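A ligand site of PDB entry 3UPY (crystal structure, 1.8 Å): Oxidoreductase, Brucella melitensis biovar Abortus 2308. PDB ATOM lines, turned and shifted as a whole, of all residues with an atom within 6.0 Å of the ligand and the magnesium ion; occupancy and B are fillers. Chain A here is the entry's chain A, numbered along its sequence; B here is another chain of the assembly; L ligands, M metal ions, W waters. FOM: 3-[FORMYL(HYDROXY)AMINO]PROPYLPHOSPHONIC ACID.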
ATOM      1  N   GLY A 166     -24.695  -5.457  13.200  1.00  0.00           N
ATOM      2  CA  GLY A 166     -25.003  -6.178  14.432  1.00  0.00           C
ATOM      3  C   GLY A 166     -24.989  -5.286  15.688  1.00  0.00           C
ATOM      4  O   GLY A 166     -25.516  -5.666  16.724  1.00  0.00           O
ATOM      5  N   ASP A 167     -24.404  -4.086  15.612  1.00  0.00           N
ATOM      6  CA  ASP A 167     -24.450  -3.162  16.746  1.00  0.00           C
ATOM      7  C   ASP A 167     -25.529  -2.104  16.433  1.00  0.00           C
ATOM      8  O   ASP A 167     -25.884  -1.925  15.271  1.00  0.00           O
ATOM      9  CB  ASP A 167     -23.072  -2.525  16.918  1.00  0.00           C
ATOM     10  CG  ASP A 167     -22.834  -1.912  18.269  1.00  0.00           C
ATOM     11  OD1 ASP A 167     -23.543  -2.122  19.243  1.00  0.00           O
ATOM     12  OD2 ASP A 167     -21.816  -1.152  18.344  1.00  0.00           O
ATOM     13  N   GLU A 168     -26.012  -1.392  17.454  1.00  0.00           N
ATOM     14  CA  GLU A 168     -27.185  -0.511  17.274  1.00  0.00           C
ATOM     15  C   GLU A 168     -27.031   0.469  16.133  1.00  0.00           C
ATOM     16  O   GLU A 168     -27.969   0.657  15.344  1.00  0.00           O
ATOM     17  CB  GLU A 168     -27.601   0.177  18.599  1.00  0.00           C
ATOM     18  CG  GLU A 168     -28.171  -0.774  19.627  1.00  0.00           C
ATOM     19  CD  GLU A 168     -27.130  -1.225  20.649  1.00  0.00           C
ATOM     20  OE1 GLU A 168     -25.949  -1.485  20.208  1.00  0.00           O
ATOM     21  OE2 GLU A 168     -27.479  -1.358  21.835  1.00  0.00           O
ATOM     22  N   PRO A 169     -25.847   1.078  15.962  1.00  0.00           N
ATOM     23  CA  PRO A 169     -25.817   2.086  14.874  1.00  0.00           C
ATOM     24  C   PRO A 169     -26.008   1.502  13.495  1.00  0.00           C
ATOM     25  O   PRO A 169     -26.755   2.047  12.681  1.00  0.00           O
ATOM     26  CB  PRO A 169     -24.417   2.730  14.976  1.00  0.00           C
ATOM     27  CG  PRO A 169     -23.871   2.311  16.275  1.00  0.00           C
ATOM     28  CD  PRO A 169     -24.564   1.040  16.707  1.00  0.00           C
ATOM     29  N   LYS A 191     -32.151   3.941  19.889  1.00  0.00           N
ATOM     30  CA  LYS A 191     -32.126   2.650  20.582  1.00  0.00           C
ATOM     31  C   LYS A 191     -32.891   2.797  21.918  1.00  0.00           C
ATOM     32  O   LYS A 191     -33.172   3.936  22.316  1.00  0.00           O
ATOM     33  CB  LYS A 191     -30.676   2.255  20.846  1.00  0.00           C
ATOM     34  CG  LYS A 191     -29.947   3.220  21.757  1.00  0.00           C
ATOM     35  CD  LYS A 191     -28.492   2.829  22.071  1.00  0.00           C
ATOM     36  CE  LYS A 191     -28.431   1.631  23.055  1.00  0.00           C
ATOM     37  NZ  LYS A 191     -27.083   1.302  23.708  1.00  0.00           N
ATOM     38  N   GLY A 192     -33.249   1.715  22.576  1.00  0.00           N
ATOM     39  CA  GLY A 192     -33.831   1.837  23.958  1.00  0.00           C
ATOM     40  C   GLY A 192     -32.938   1.392  25.158  1.00  0.00           C
ATOM     41  O   GLY A 192     -31.949   0.747  24.980  1.00  0.00           O
ATOM     42  N   LYS A 193     -33.334   1.778  26.362  1.00  0.00           N
ATOM     43  CA  LYS A 193     -32.782   1.192  27.621  1.00  0.00           C
ATOM     44  C   LYS A 193     -33.893   0.892  28.616  1.00  0.00           C
ATOM     45  O   LYS A 193     -34.810   1.735  28.851  1.00  0.00           O
ATOM     46  CB  LYS A 193     -31.786   2.138  28.275  1.00  0.00           C
ATOM     47  CG  LYS A 193     -30.538   2.424  27.439  1.00  0.00           C
ATOM     48  CD  LYS A 193     -29.279   1.742  27.994  1.00  0.00           C
ATOM     49  CE  LYS A 193     -28.632   2.581  29.108  1.00  0.00           C
ATOM     50  NZ  LYS A 193     -27.450   1.852  29.790  1.00  0.00           N
ATOM     51  N   GLU A 222     -19.763   1.619  31.318  1.00  0.00           N
ATOM     52  CA  GLU A 222     -19.981   2.537  30.197  1.00  0.00           C
ATOM     53  C   GLU A 222     -21.361   2.319  29.567  1.00  0.00           C
ATOM     54  O   GLU A 222     -21.866   3.194  28.902  1.00  0.00           O
ATOM     55  CB  GLU A 222     -18.891   2.305  29.174  1.00  0.00           C
ATOM     56  CG  GLU A 222     -19.118   1.146  28.399  1.00  0.00           C
ATOM     57  CD  GLU A 222     -18.257   0.963  27.184  1.00  0.00           C
ATOM     58  OE1 GLU A 222     -18.307  -0.205  26.750  1.00  0.00           O
ATOM     59  OE2 GLU A 222     -17.651   1.918  26.608  1.00  0.00           O
ATOM     60  N   PHE A 223     -21.929   1.164  29.836  1.00  0.00           N
ATOM     61  CA  PHE A 223     -23.290   0.882  29.478  1.00  0.00           C
ATOM     62  C   PHE A 223     -24.230   1.709  30.460  1.00  0.00           C
ATOM     63  O   PHE A 223     -24.994   2.500  30.063  1.00  0.00           O
ATOM     64  CB  PHE A 223     -23.583  -0.669  29.501  1.00  0.00           C
ATOM     65  CG  PHE A 223     -22.706  -1.561  28.524  1.00  0.00           C
ATOM     66  CD1 PHE A 223     -21.931  -1.039  27.500  1.00  0.00           C
ATOM     67  CD2 PHE A 223     -22.713  -2.972  28.630  1.00  0.00           C
ATOM     68  CE1 PHE A 223     -21.200  -1.811  26.673  1.00  0.00           C
ATOM     69  CE2 PHE A 223     -21.965  -3.792  27.763  1.00  0.00           C
ATOM     70  CZ  PHE A 223     -21.218  -3.218  26.760  1.00  0.00           C
ATOM     71  N   ILE A 224     -24.094   1.498  31.766  1.00  0.00           N
ATOM     72  CA  ILE A 224     -24.902   2.134  32.787  1.00  0.00           C
ATOM     73  C   ILE A 224     -24.750   3.658  32.863  1.00  0.00           C
ATOM     74  O   ILE A 224     -25.726   4.382  33.137  1.00  0.00           O
ATOM     75  CB  ILE A 224     -24.541   1.546  34.232  1.00  0.00           C
ATOM     76  CG1 ILE A 224     -24.911   0.068  34.398  1.00  0.00           C
ATOM     77  CG2 ILE A 224     -25.192   2.363  35.209  1.00  0.00           C
ATOM     78  CD1 ILE A 224     -26.472  -0.225  34.650  1.00  0.00           C
ATOM     79  N   LYS A 228     -21.772   4.468  26.210  1.00  0.00           N
ATOM     80  CA  LYS A 228     -21.992   3.705  24.995  1.00  0.00           C
ATOM     81  C   LYS A 228     -23.193   4.213  24.147  1.00  0.00           C
ATOM     82  O   LYS A 228     -23.133   4.264  22.901  1.00  0.00           O
ATOM     83  CB  LYS A 228     -22.248   2.261  25.368  1.00  0.00           C
ATOM     84  CG  LYS A 228     -22.411   1.348  24.170  1.00  0.00           C
ATOM     85  CD  LYS A 228     -21.157   1.346  23.276  1.00  0.00           C
ATOM     86  CE  LYS A 228     -20.088   0.429  23.685  1.00  0.00           C
ATOM     87  NZ  LYS A 228     -19.095   0.563  22.582  1.00  0.00           N
ATOM     88  N   THR A 229     -24.258   4.615  24.824  1.00  0.00           N
ATOM     89  CA  THR A 229     -25.403   5.195  24.171  1.00  0.00           C
ATOM     90  C   THR A 229     -25.067   6.503  23.426  1.00  0.00           C
ATOM     91  O   THR A 229     -25.523   6.710  22.282  1.00  0.00           O
ATOM     92  CB  THR A 229     -26.602   5.356  25.119  1.00  0.00           C
ATOM     93  OG1 THR A 229     -27.052   4.024  25.491  1.00  0.00           O
ATOM     94  CG2 THR A 229     -27.745   6.128  24.465  1.00  0.00           C
ATOM     95  N   GLU A 232     -22.951   5.487  20.300  1.00  0.00           N
ATOM     96  CA  GLU A 232     -23.763   4.809  19.266  1.00  0.00           C
ATOM     97  C   GLU A 232     -24.683   5.797  18.551  1.00  0.00           C
ATOM     98  O   GLU A 232     -24.849   5.741  17.308  1.00  0.00           O
ATOM     99  CB  GLU A 232     -24.594   3.695  19.866  1.00  0.00           C
ATOM    100  CG  GLU A 232     -23.712   2.484  20.105  1.00  0.00           C
ATOM    101  CD  GLU A 232     -24.395   1.318  20.834  1.00  0.00           C
ATOM    102  OE1 GLU A 232     -25.552   1.395  21.258  1.00  0.00           O
ATOM    103  OE2 GLU A 232     -23.706   0.298  21.017  1.00  0.00           O
ATOM    104  N   HIS A 323     -30.514  -7.187  17.637  1.00  0.00           N
ATOM    105  CA  HIS A 323     -29.217  -6.850  17.002  1.00  0.00           C
ATOM    106  C   HIS A 323     -28.304  -7.972  17.575  1.00  0.00           C
ATOM    107  O   HIS A 323     -28.422  -8.208  18.727  1.00  0.00           O
ATOM    108  CB  HIS A 323     -28.754  -5.403  17.359  1.00  0.00           C
ATOM    109  CG  HIS A 323     -28.321  -5.187  18.794  1.00  0.00           C
ATOM    110  ND1 HIS A 323     -29.193  -5.178  19.863  1.00  0.00           N
ATOM    111  CD2 HIS A 323     -27.094  -4.949  19.313  1.00  0.00           C
ATOM    112  CE1 HIS A 323     -28.517  -4.950  20.979  1.00  0.00           C
ATOM    113  NE2 HIS A 323     -27.231  -4.802  20.662  1.00  0.00           N
ATOM    114  N   THR A 325     -24.887  -8.223  17.699  1.00  0.00           N
ATOM    115  CA  THR A 325     -23.518  -7.763  17.927  1.00  0.00           C
ATOM    116  C   THR A 325     -22.541  -8.455  16.965  1.00  0.00           C
ATOM    117  O   THR A 325     -22.783  -8.484  15.734  1.00  0.00           O
ATOM    118  CB  THR A 325     -23.110  -7.846  19.427  1.00  0.00           C
ATOM    119  OG1 THR A 325     -23.015  -9.234  19.851  1.00  0.00           O
ATOM    120  CG2 THR A 325     -24.139  -7.075  20.288  1.00  0.00           C
ATOM    121  N   LEU B 308     -27.930 -10.940  25.363  1.00  0.00           N
ATOM    122  CA  LEU B 308     -28.594  -9.849  24.652  1.00  0.00           C
ATOM    123  C   LEU B 308     -30.113  -9.812  24.899  1.00  0.00           C
ATOM    124  O   LEU B 308     -30.773  -8.875  24.457  1.00  0.00           O
ATOM    125  CB  LEU B 308     -28.310  -9.946  23.162  1.00  0.00           C
ATOM    126  CG  LEU B 308     -26.840  -9.688  22.778  1.00  0.00           C
ATOM    127  CD1 LEU B 308     -26.529 -10.175  21.395  1.00  0.00           C
ATOM    128  CD2 LEU B 308     -26.605  -8.206  22.882  1.00  0.00           C
HETATM  129  O2  FOM L   1     -25.124  -1.491  22.886  1.00  0.00           O
HETATM  130  N1  FOM L   1     -25.146  -2.697  23.244  1.00  0.00           N
HETATM  131  C1  FOM L   1     -24.909  -3.726  22.477  1.00  0.00           C
HETATM  132  O1  FOM L   1     -24.506  -3.562  21.328  1.00  0.00           O
HETATM  133  C2  FOM L   1     -25.442  -3.030  24.609  1.00  0.00           C
HETATM  134  C3  FOM L   1     -24.720  -2.096  25.538  1.00  0.00           C
HETATM  135  C4  FOM L   1     -25.671  -1.855  26.687  1.00  0.00           C
HETATM  136  PA1 FOM L   1     -26.536  -0.290  26.524  1.00  0.00           P
HETATM  137  OP1 FOM L   1     -25.605   0.898  26.147  1.00  0.00           O
HETATM  138  OP2 FOM L   1     -27.540  -0.662  25.392  1.00  0.00           O
HETATM  139  OP3 FOM L   1     -27.103  -0.249  27.971  1.00  0.00           O
HETATM  140 MG    MG M   1     -24.200  -1.696  21.114  1.00  0.00          MG
HETATM  141  O   HOH W   1     -21.530  -4.279  20.500  1.00  0.00           O
HETATM  142  O   HOH W   2     -22.456  -2.093  22.140  1.00  0.00           O
HETATM  143  O   HOH W   3     -25.029   3.280  27.467  1.00  0.00           O
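NZ of Lys 191 lies within salt-bridge range of OP2 of the ligand, at 2.6 Å.
A ring nitrogen (NE2) of His 323 sits close to an oxygen (O1) of the ligand (3.1 Å).
OP3 of the ligand is in salt-bridge range of NZ of Lys 193 (2.8 Å).
The side-chain carboxylate (OE1) of Glu 232 lies within salt-bridge range of the side-chain amino group (NZ) of Lys 191 (2.9 Å).
The side-chain amino group (NZ) of Lys 193 is in hydrogen-bond range of the backbone carbonyl oxygen (O) of Phe 223, at 2.6 Å.
The backbone carbonyl oxygen (O) of Gly 166 sits at hydrogen-bond distance from the backbone NH (N) of Thr 325, 2.8 Å away.
The backbone carbonyl oxygen of Glu 222 is in hydrogen-bond range of the backbone NH of Lys 228 (3.0 Å).
The side-chain amino group (NZ) of Lys 191 sits at hydrogen-bond distance from the side-chain hydroxyl (OG1) of Thr 229 (3.3 Å).
The side-chain carboxylate (OE2) of Glu 168 is in salt-bridge range of the side-chain amino group (NZ) of Lys 191 (3.3 Å).
Merely in contact with the ligand: Phe 223, Thr 229, Thr 325 and Lys 228.
Within 4 Å of the ligand: Asp 167, Glu 168, Lys 191, Lys 193, Phe 223, Lys 228, Thr 229, Glu 232, His 323 and Thr 325.
Within 4 Å of the magnesium ion: Asp 167, Glu 168 and Glu 232.
The nearest printed residue that does not touch the magnesium ion is His 323 (4.4 Å).
The magnesium ion is bound by O1 of the ligand (1.9 Å).
The magnesium ion is bound by the side-chain carboxylate (OE1) of Glu 168 (2.0 Å).
O2 of the ligand binds the magnesium ion (2.0 Å).
The magnesium ion is bound by OD1 of Asp 167 (2.0 Å).
The magnesium ion is bound by OE2 of Glu 232, 2.1 Å away.
Water W2 is bound to the magnesium ion, 2.1 Å away.
Water W3 lies within hydrogen-bond range of O of Phe 223 (2.7 Å), OP1 of the ligand (2.8 Å), OG1 of Thr 229 (2.9 Å) and O of Glu 222 (3.5 Å).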
